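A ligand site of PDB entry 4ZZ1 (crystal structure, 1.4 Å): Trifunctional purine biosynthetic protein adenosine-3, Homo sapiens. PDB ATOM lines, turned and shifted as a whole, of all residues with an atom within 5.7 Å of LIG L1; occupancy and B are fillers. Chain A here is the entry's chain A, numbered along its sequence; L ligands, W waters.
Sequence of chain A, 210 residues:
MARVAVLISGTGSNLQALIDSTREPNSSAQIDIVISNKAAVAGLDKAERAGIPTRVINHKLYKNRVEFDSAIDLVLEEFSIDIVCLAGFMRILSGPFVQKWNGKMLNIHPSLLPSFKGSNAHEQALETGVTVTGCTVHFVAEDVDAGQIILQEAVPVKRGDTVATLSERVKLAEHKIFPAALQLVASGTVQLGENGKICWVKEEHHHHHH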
ATOM      1  N   GLY A  10     -12.530  22.125   8.290  1.00  0.00           N
ATOM      2  CA  GLY A  10     -11.259  22.265   7.607  1.00  0.00           C
ATOM      3  C   GLY A  10     -10.570  23.612   7.692  1.00  0.00           C
ATOM      4  O   GLY A  10     -10.339  24.130   8.789  1.00  0.00           O
ATOM      5  N   THR A  11     -10.252  24.164   6.534  1.00  0.00           N
ATOM      6  CA  THR A  11      -9.382  25.330   6.407  1.00  0.00           C
ATOM      7  C   THR A  11      -9.908  26.577   7.131  1.00  0.00           C
ATOM      8  O   THR A  11      -9.150  27.280   7.798  1.00  0.00           O
ATOM      9  CB  THR A  11      -9.158  25.648   4.921  1.00  0.00           C
ATOM     10  OG1 THR A  11      -8.558  24.517   4.291  1.00  0.00           O
ATOM     11  CG2 THR A  11      -8.246  26.863   4.744  1.00  0.00           C
ATOM     12  N   GLY A  12     -11.199  26.847   6.985  1.00  0.00           N
ATOM     13  CA  GLY A  12     -11.824  27.928   7.707  1.00  0.00           C
ATOM     14  C   GLY A  12     -11.753  29.294   7.057  1.00  0.00           C
ATOM     15  O   GLY A  12     -11.852  30.314   7.750  1.00  0.00           O
ATOM     16  N   SER A  13     -11.611  29.342   5.735  1.00  0.00           N
ATOM     17  CA  SER A  13     -11.653  30.641   5.051  1.00  0.00           C
ATOM     18  C   SER A  13     -13.033  31.298   5.192  1.00  0.00           C
ATOM     19  O   SER A  13     -13.116  32.514   5.375  1.00  0.00           O
ATOM     20  CB  SER A  13     -11.269  30.522   3.570  1.00  0.00           C
ATOM     21  OG  SER A  13     -12.270  29.888   2.784  1.00  0.00           O
ATOM     22  N   ASN A  14     -14.101  30.518   5.136  1.00  0.00           N
ATOM     23  CA  ASN A  14     -15.419  31.099   5.357  1.00  0.00           C
ATOM     24  C   ASN A  14     -15.558  31.601   6.798  1.00  0.00           C
ATOM     25  O   ASN A  14     -16.099  32.680   7.038  1.00  0.00           O
ATOM     26  CB  ASN A  14     -16.536  30.105   5.036  1.00  0.00           C
ATOM     27  CG  ASN A  14     -16.908  30.126   3.567  1.00  0.00           C
ATOM     28  OD1 ASN A  14     -17.565  31.043   3.093  1.00  0.00           O
ATOM     29  ND2 ASN A  14     -16.487  29.104   2.839  1.00  0.00           N
ATOM     30  N   LEU A  15     -15.058  30.823   7.761  1.00  0.00           N
ATOM     31  CA  LEU A  15     -15.017  31.264   9.142  1.00  0.00           C
ATOM     32  C   LEU A  15     -14.302  32.606   9.263  1.00  0.00           C
ATOM     33  O   LEU A  15     -14.801  33.509   9.932  1.00  0.00           O
ATOM     34  CB  LEU A  15     -14.335  30.218  10.025  1.00  0.00           C
ATOM     35  CG  LEU A  15     -13.955  30.671  11.437  1.00  0.00           C
ATOM     36  CD1 LEU A  15     -15.188  31.059  12.246  1.00  0.00           C
ATOM     37  CD2 LEU A  15     -13.173  29.570  12.113  1.00  0.00           C
ATOM     38  N   ALA A  87     -19.871  26.128   7.933  1.00  0.00           N
ATOM     39  CA  ALA A  87     -18.874  26.827   7.118  1.00  0.00           C
ATOM     40  C   ALA A  87     -17.759  25.852   6.782  1.00  0.00           C
ATOM     41  O   ALA A  87     -16.765  25.755   7.496  1.00  0.00           O
ATOM     42  CB  ALA A  87     -18.330  28.053   7.865  1.00  0.00           C
ATOM     43  N   GLY A  88     -17.945  25.092   5.712  1.00  0.00           N
ATOM     44  CA  GLY A  88     -17.052  23.997   5.414  1.00  0.00           C
ATOM     45  C   GLY A  88     -17.238  22.782   6.313  1.00  0.00           C
ATOM     46  O   GLY A  88     -16.411  21.892   6.310  1.00  0.00           O
ATOM     47  N   PHE A  89     -18.339  22.761   7.070  1.00  0.00           N
ATOM     48  CA  PHE A  89     -18.701  21.608   7.890  1.00  0.00           C
ATOM     49  C   PHE A  89     -19.255  20.504   6.991  1.00  0.00           C
ATOM     50  O   PHE A  89     -20.188  20.757   6.218  1.00  0.00           O
ATOM     51  CB  PHE A  89     -19.724  22.048   8.927  1.00  0.00           C
ATOM     52  CG  PHE A  89     -20.130  20.968   9.890  1.00  0.00           C
ATOM     53  CD1 PHE A  89     -19.295  20.568  10.920  1.00  0.00           C
ATOM     54  CD2 PHE A  89     -21.386  20.371   9.783  1.00  0.00           C
ATOM     55  CE1 PHE A  89     -19.692  19.592  11.825  1.00  0.00           C
ATOM     56  CE2 PHE A  89     -21.788  19.393  10.664  1.00  0.00           C
ATOM     57  CZ  PHE A  89     -20.938  19.001  11.690  1.00  0.00           C
ATOM     58  N   MET A  90     -18.711  19.297   7.077  1.00  0.00           N
ATOM     59  CA  MET A  90     -19.015  18.303   6.042  1.00  0.00           C
ATOM     60  C   MET A  90     -19.900  17.144   6.507  1.00  0.00           C
ATOM     61  O   MET A  90     -20.051  16.161   5.761  1.00  0.00           O
ATOM     62  CB  MET A  90     -17.713  17.773   5.441  1.00  0.00           C
ATOM     63  CG  MET A  90     -16.963  18.791   4.584  1.00  0.00           C
ATOM     64  SD  MET A  90     -17.943  19.516   3.229  1.00  0.00           S
ATOM     65  CE  MET A  90     -18.404  18.045   2.326  1.00  0.00           C
ATOM     66  N   ASN A 107     -26.188  27.277   5.810  1.00  0.00           N
ATOM     67  CA  ASN A 107     -25.104  26.542   5.181  1.00  0.00           C
ATOM     68  C   ASN A 107     -24.603  27.269   3.952  1.00  0.00           C
ATOM     69  O   ASN A 107     -25.407  27.894   3.244  1.00  0.00           O
ATOM     70  CB  ASN A 107     -25.566  25.131   4.813  1.00  0.00           C
ATOM     71  CG  ASN A 107     -24.478  24.303   4.181  1.00  0.00           C
ATOM     72  OD1 ASN A 107     -23.420  24.094   4.766  1.00  0.00           O
ATOM     73  ND2 ASN A 107     -24.748  23.802   2.965  1.00  0.00           N
ATOM     74  N   ILE A 108     -23.298  27.189   3.681  1.00  0.00           N
ATOM     75  CA  ILE A 108     -22.752  27.662   2.396  1.00  0.00           C
ATOM     76  C   ILE A 108     -22.398  26.450   1.544  1.00  0.00           C
ATOM     77  O   ILE A 108     -21.829  25.461   2.020  1.00  0.00           O
ATOM     78  CB  ILE A 108     -21.521  28.595   2.604  1.00  0.00           C
ATOM     79  CG1 ILE A 108     -21.011  29.123   1.269  1.00  0.00           C
ATOM     80  CG2 ILE A 108     -20.377  27.897   3.294  1.00  0.00           C
ATOM     81  CD1 ILE A 108     -21.725  30.302   0.741  1.00  0.00           C
ATOM     82  N   HIS A 109     -22.778  26.528   0.278  1.00  0.00           N
ATOM     83  CA  HIS A 109     -22.591  25.423  -0.654  1.00  0.00           C
ATOM     84  C   HIS A 109     -21.972  25.991  -1.924  1.00  0.00           C
ATOM     85  O   HIS A 109     -22.473  26.986  -2.440  1.00  0.00           O
ATOM     86  CB  HIS A 109     -23.927  24.744  -0.940  1.00  0.00           C
ATOM     87  CG  HIS A 109     -23.780  23.576  -1.846  1.00  0.00           C
ATOM     88  ND1 HIS A 109     -23.382  22.336  -1.393  1.00  0.00           N
ATOM     89  CD2 HIS A 109     -23.933  23.466  -3.187  1.00  0.00           C
ATOM     90  CE1 HIS A 109     -23.304  21.507  -2.424  1.00  0.00           C
ATOM     91  NE2 HIS A 109     -23.640  22.170  -3.523  1.00  0.00           N
ATOM     92  N   PRO A 110     -20.901  25.356  -2.439  1.00  0.00           N
ATOM     93  CA  PRO A 110     -20.172  25.944  -3.574  1.00  0.00           C
ATOM     94  C   PRO A 110     -20.751  25.566  -4.945  1.00  0.00           C
ATOM     95  O   PRO A 110     -20.017  25.139  -5.837  1.00  0.00           O
ATOM     96  CB  PRO A 110     -18.753  25.387  -3.388  1.00  0.00           C
ATOM     97  CG  PRO A 110     -19.009  24.006  -2.814  1.00  0.00           C
ATOM     98  CD  PRO A 110     -20.204  24.183  -1.883  1.00  0.00           C
ATOM     99  N   GLY A 118     -24.382  18.069  -2.949  1.00  0.00           N
ATOM    100  CA  GLY A 118     -23.496  17.040  -2.454  1.00  0.00           C
ATOM    101  C   GLY A 118     -22.100  17.533  -2.124  1.00  0.00           C
ATOM    102  O   GLY A 118     -21.860  18.733  -2.001  1.00  0.00           O
ATOM    103  N   SER A 119     -21.160  16.592  -1.977  1.00  0.00           N
ATOM    104  CA  SER A 119     -19.871  16.909  -1.383  1.00  0.00           C
ATOM    105  C   SER A 119     -18.792  17.324  -2.364  1.00  0.00           C
ATOM    106  O   SER A 119     -17.730  17.801  -1.949  1.00  0.00           O
ATOM    107  CB  SER A 119     -19.351  15.694  -0.601  1.00  0.00           C
ATOM    108  OG  SER A 119     -19.130  14.621  -1.493  1.00  0.00           O
ATOM    109  N   HIS A 122     -17.715  21.112  -7.204  1.00  0.00           N
ATOM    110  CA  HIS A 122     -16.825  21.582  -8.278  1.00  0.00           C
ATOM    111  C   HIS A 122     -16.526  20.476  -9.276  1.00  0.00           C
ATOM    112  O   HIS A 122     -16.500  20.721 -10.473  1.00  0.00           O
ATOM    113  CB  HIS A 122     -15.524  22.132  -7.718  1.00  0.00           C
ATOM    114  CG  HIS A 122     -15.712  23.319  -6.824  1.00  0.00           C
ATOM    115  ND1 HIS A 122     -16.366  24.459  -7.229  1.00  0.00           N
ATOM    116  CD2 HIS A 122     -15.330  23.514  -5.542  1.00  0.00           C
ATOM    117  CE1 HIS A 122     -16.369  25.321  -6.229  1.00  0.00           C
ATOM    118  NE2 HIS A 122     -15.753  24.771  -5.193  1.00  0.00           N
ATOM    119  N   ASP A 145     -28.952  20.130   1.185  1.00  0.00           N
ATOM    120  CA  ASP A 145     -28.748  21.138   0.144  1.00  0.00           C
ATOM    121  C   ASP A 145     -30.052  21.525  -0.550  1.00  0.00           C
ATOM    122  O   ASP A 145     -30.038  21.970  -1.699  1.00  0.00           O
ATOM    123  CB  ASP A 145     -27.726  20.648  -0.897  1.00  0.00           C
ATOM    124  CG  ASP A 145     -26.335  20.465  -0.297  1.00  0.00           C
ATOM    125  OD1 ASP A 145     -26.048  21.071   0.761  1.00  0.00           O
ATOM    126  OD2 ASP A 145     -25.515  19.740  -0.908  1.00  0.00           O
ATOM    127  N   SER A 167     -12.419  26.348  -7.221  1.00  0.00           N
ATOM    128  CA  SER A 167     -12.794  26.524  -5.822  1.00  0.00           C
ATOM    129  C   SER A 167     -12.224  27.822  -5.269  1.00  0.00           C
ATOM    130  O   SER A 167     -12.897  28.514  -4.491  1.00  0.00           O
ATOM    131  CB  SER A 167     -12.349  25.329  -4.975  1.00  0.00           C
ATOM    132  OG  SER A 167     -10.940  25.238  -4.883  1.00  0.00           O
ATOM    133  N   LYS A 171     -14.653  30.674  -3.762  1.00  0.00           N
ATOM    134  CA  LYS A 171     -14.521  31.099  -2.374  1.00  0.00           C
ATOM    135  C   LYS A 171     -14.521  32.618  -2.212  1.00  0.00           C
ATOM    136  O   LYS A 171     -14.993  33.115  -1.196  1.00  0.00           O
ATOM    137  CB  LYS A 171     -13.263  30.504  -1.728  1.00  0.00           C
ATOM    138  CG  LYS A 171     -13.490  29.080  -1.267  1.00  0.00           C
ATOM    139  CD  LYS A 171     -12.266  28.476  -0.642  1.00  0.00           C
ATOM    140  CE  LYS A 171     -12.551  27.034  -0.263  1.00  0.00           C
ATOM    141  NZ  LYS A 171     -11.449  26.490   0.573  1.00  0.00           N
ATOM    142  N   GLU A 174     -18.067  33.226  -1.912  1.00  0.00           N
ATOM    143  CA  GLU A 174     -18.584  32.690  -0.654  1.00  0.00           C
ATOM    144  C   GLU A 174     -18.340  33.655   0.483  1.00  0.00           C
ATOM    145  O   GLU A 174     -19.194  33.858   1.348  1.00  0.00           O
ATOM    146  CB  GLU A 174     -17.932  31.352  -0.316  1.00  0.00           C
ATOM    147  CG  GLU A 174     -18.254  30.240  -1.276  1.00  0.00           C
ATOM    148  CD  GLU A 174     -17.537  28.967  -0.914  1.00  0.00           C
ATOM    149  OE1 GLU A 174     -17.285  28.735   0.285  1.00  0.00           O
ATOM    150  OE2 GLU A 174     -17.204  28.181  -1.831  1.00  0.00           O
ATOM    151  N   HIS A 175     -17.152  34.254   0.479  1.00  0.00           N
ATOM    152  CA  HIS A 175     -16.760  35.182   1.532  1.00  0.00           C
ATOM    153  C   HIS A 175     -17.510  36.492   1.497  1.00  0.00           C
ATOM    154  O   HIS A 175     -17.397  37.284   2.430  1.00  0.00           O
ATOM    155  CB  HIS A 175     -15.260  35.438   1.457  1.00  0.00           C
ATOM    156  CG  HIS A 175     -14.437  34.202   1.594  1.00  0.00           C
ATOM    157  ND1 HIS A 175     -13.120  34.143   1.198  1.00  0.00           N
ATOM    158  CD2 HIS A 175     -14.755  32.971   2.037  1.00  0.00           C
ATOM    159  CE1 HIS A 175     -12.651  32.921   1.409  1.00  0.00           C
ATOM    160  NE2 HIS A 175     -13.630  32.184   1.913  1.00  0.00           N
HETATM  161  C1  LIG L   1     -16.185  25.864   0.871  1.00  0.00           C
HETATM  162  O1  LIG L   1     -15.969  25.942  -0.552  1.00  0.00           O
HETATM  163  C2  LIG L   1     -17.610  25.460   1.165  1.00  0.00           C
HETATM  164  O2  LIG L   1     -18.625  26.074   0.344  1.00  0.00           O
HETATM  165  C3  LIG L   1     -17.532  23.963   0.930  1.00  0.00           C
HETATM  166  O3  LIG L   1     -16.321  23.609   1.567  1.00  0.00           O
HETATM  167  C4  LIG L   1     -15.389  24.688   1.436  1.00  0.00           C
HETATM  168  C5  LIG L   1     -14.872  24.998   2.841  1.00  0.00           C
HETATM  169  O4  LIG L   1     -13.820  25.953   2.756  1.00  0.00           O
HETATM  170  N1  LIG L   1     -18.633  23.267   1.549  1.00  0.00           N
HETATM  171  C6  LIG L   1     -19.189  22.184   1.014  1.00  0.00           C
HETATM  172  O5  LIG L   1     -18.763  21.605   0.010  1.00  0.00           O
HETATM  173  C7  LIG L   1     -20.433  21.741   1.756  1.00  0.00           C
HETATM  174  N2  LIG L   1     -20.985  20.505   1.276  1.00  0.00           N
HETATM  175  P1  LIG L   1     -13.331  26.717   4.104  1.00  0.00           P
HETATM  176  O6  LIG L   1     -14.459  27.642   4.492  1.00  0.00           O
HETATM  177  O7  LIG L   1     -12.078  27.439   3.634  1.00  0.00           O
HETATM  178  O8  LIG L   1     -13.062  25.650   5.152  1.00  0.00           O
HETATM  179  N1  LG2 L   2     -27.511  18.278   6.900  1.00  0.00           N
HETATM  180  C1  LG2 L   2     -28.784  18.352   6.533  1.00  0.00           C
HETATM  181  N2  LG2 L   2     -29.212  19.223   5.603  1.00  0.00           N
HETATM  182  C2  LG2 L   2     -28.376  20.090   5.000  1.00  0.00           C
HETATM  183  N3  LG2 L   2     -25.287  19.227   6.551  1.00  0.00           N
HETATM  184  C3  LG2 L   2     -24.775  20.178   5.783  1.00  0.00           C
HETATM  185  C4  LG2 L   2     -25.802  20.750   5.009  1.00  0.00           C
HETATM  186  C5  LG2 L   2     -26.988  20.053   5.370  1.00  0.00           C
HETATM  187  C6  LG2 L   2     -26.596  19.113   6.354  1.00  0.00           C
HETATM  188  O1  LG2 L   2     -28.778  20.890   4.153  1.00  0.00           O
HETATM  189  N4  LG2 L   2     -29.704  17.482   7.116  1.00  0.00           N
HETATM  190  C7  LG2 L   2     -22.476  16.559   3.465  1.00  0.00           C
HETATM  191  C8  LG2 L   2     -22.226  15.490   2.647  1.00  0.00           C
HETATM  192  S1  LG2 L   2     -22.672  15.983   1.084  1.00  0.00           S
HETATM  193  C9  LG2 L   2     -23.172  17.565   1.488  1.00  0.00           C
HETATM  194  C10 LG2 L   2     -22.997  17.726   2.842  1.00  0.00           C
HETATM  195  C11 LG2 L   2     -21.707  14.200   2.990  1.00  0.00           C
HETATM  196  O2  LG2 L   2     -21.757  13.268   2.165  1.00  0.00           O
HETATM  197  N5  LG2 L   2     -21.135  14.022   4.293  1.00  0.00           N
HETATM  198  C12 LG2 L   2     -20.624  12.728   4.646  1.00  0.00           C
HETATM  199  C13 LG2 L   2     -19.177  12.855   4.968  1.00  0.00           C
HETATM  200  C14 LG2 L   2     -18.353  12.986   3.691  1.00  0.00           C
HETATM  201  C15 LG2 L   2     -16.935  13.550   3.966  1.00  0.00           C
HETATM  202  O3  LG2 L   2     -16.386  14.347   3.115  1.00  0.00           O
HETATM  203  O4  LG2 L   2     -16.302  13.215   5.060  1.00  0.00           O
HETATM  204  C16 LG2 L   2     -21.406  12.252   5.869  1.00  0.00           C
HETATM  205  O5  LG2 L   2     -21.570  10.972   6.065  1.00  0.00           O
HETATM  206  O6  LG2 L   2     -21.912  13.111   6.684  1.00  0.00           O
HETATM  207  C17 LG2 L   2     -23.261  20.503   5.751  1.00  0.00           C
HETATM  208  C18 LG2 L   2     -22.610  19.313   4.921  1.00  0.00           C
HETATM  209  C19 LG2 L   2     -23.362  19.001   3.601  1.00  0.00           C
HETATM  210  O   HOH W   1     -23.561  21.621   1.234  1.00  0.00           O
HETATM  211  O   HOH W   2     -14.879  27.953   7.148  1.00  0.00           O
HETATM  212  O   HOH W   3     -15.342  27.063  -3.594  1.00  0.00           O
HETATM  213  O   HOH W   4     -19.630  20.437  -2.583  1.00  0.00           O
HETATM  214  O   HOH W   5     -14.704  21.188   1.947  1.00  0.00           O
HETATM  215  O   HOH W   6     -14.218  24.401   7.336  1.00  0.00           O
HETATM  216  O   HOH W   7     -12.077  23.263   4.372  1.00  0.00           O
HETATM  217  O   HOH W   8     -19.890  24.599   3.726  1.00  0.00           O
HETATM  218  O   HOH W   9     -15.975  21.634  -1.703  1.00  0.00           O
HETATM  219  O   HOH W  10     -14.876  24.052  -2.210  1.00  0.00           O
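O7 of LIG L1 sits at hydrogen-bond distance from N of Ser 13, 2.9 Å away.
An oxygen (O7) of LIG L1 lies within hydrogen-bond range of the side-chain hydroxyl of Ser 13 (2.6 Å).
An oxygen (O1) of LIG L1 lies within hydrogen-bond range of the side-chain carboxylate of Glu 174.
The backbone NH (N) of Gly 12 is in hydrogen-bond range of an oxygen (O8) of LIG L1, 2.9 Å away.
N of Asn 14 sits at hydrogen-bond distance from O6 of LIG L1, 3.0 Å away.
The side-chain amide nitrogen of Asn 14 lies within hydrogen-bond range of an oxygen (O6) of LIG L1, at 3.0 Å.
NZ of Lys 171 lies within salt-bridge range of O7 of LIG L1 (3.3 Å).
N of Thr 11 is in hydrogen-bond range of O8 of LIG L1 (3.5 Å).
The side-chain sulfur (SD) of Met 90 sits close to a nitrogen (N2) of LIG L1 (3.7 Å).
The backbone carbonyl oxygen (O) of Met 90 is in hydrogen-bond range of a nitrogen (N5) of LG2 L2, 2.8 Å away.
The backbone NH (N) of Ser 119 sits close to a sulfur (S1) of LG2 L2, 3.5 Å away.
N of Asp 145 is in hydrogen-bond range of O1 of LG2 L2, at 3.1 Å.
The side-chain hydroxyl of Ser 13 sits at hydrogen-bond distance from a ring nitrogen (NE2) of His 175, 2.8 Å away.
OE1 of Glu 174 lies within hydrogen-bond range of ND2 of Asn 14 (2.7 Å).
The backbone carbonyl oxygen (O) of Lys 171 sits close to a ring nitrogen (ND1) of His 175 (3.2 Å).
N of Gly 118 is in hydrogen-bond range of OD2 of Asp 145.
Residues that only touch LIG L1: Gly 88 (3.5 Å), Ile 108 (3.7 Å), Pro 110 (3.3 Å) and Gly 118 (3.8 Å).
Hydrophobic or aromatic side chains that line LIG L1: Met 90, Ile 108 and Pro 110.
Of the 22 residues printed, 11 come within 4 Å of LIG L1.
Water W7 lies within hydrogen-bond range of an oxygen (O8) of LIG L1 (2.7 Å) and the backbone NH (N) of Thr 11 (3.0 Å).
Water W2 lies within hydrogen-bond range of O6 of LIG L1, O of Ala 87, N of Leu 15 and N of Asn 14.
Water W10 bridges O1 of LIG L1 (2.7 Å) and NE2 of His 122 (3.2 Å).
Water W6 lies within hydrogen-bond range of an oxygen (O8) of LIG L1 (2.8 Å), the backbone carbonyl oxygen (O) of Ala 87 (2.9 Å), the backbone NH (N) of Gly 10 (3.0 Å) and the backbone carbonyl oxygen (O) of Gly 88 (3.5 Å).
Water W1 lies within hydrogen-bond range of OD1 of Asp 145 (2.6 Å), ND1 of His 109 (2.7 Å), N2 of LIG L1 (2.8 Å) and ND2 of Asn 107 (3.0 Å).
Water W3 lies within hydrogen-bond range of the side-chain carboxylate of Glu 174 (2.8 Å), a ring nitrogen (NE2) of His 122 (2.8 Å), the backbone carbonyl oxygen of Ser 167 (3.0 Å) and an oxygen (O1) of LIG L1 (3.3 Å).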
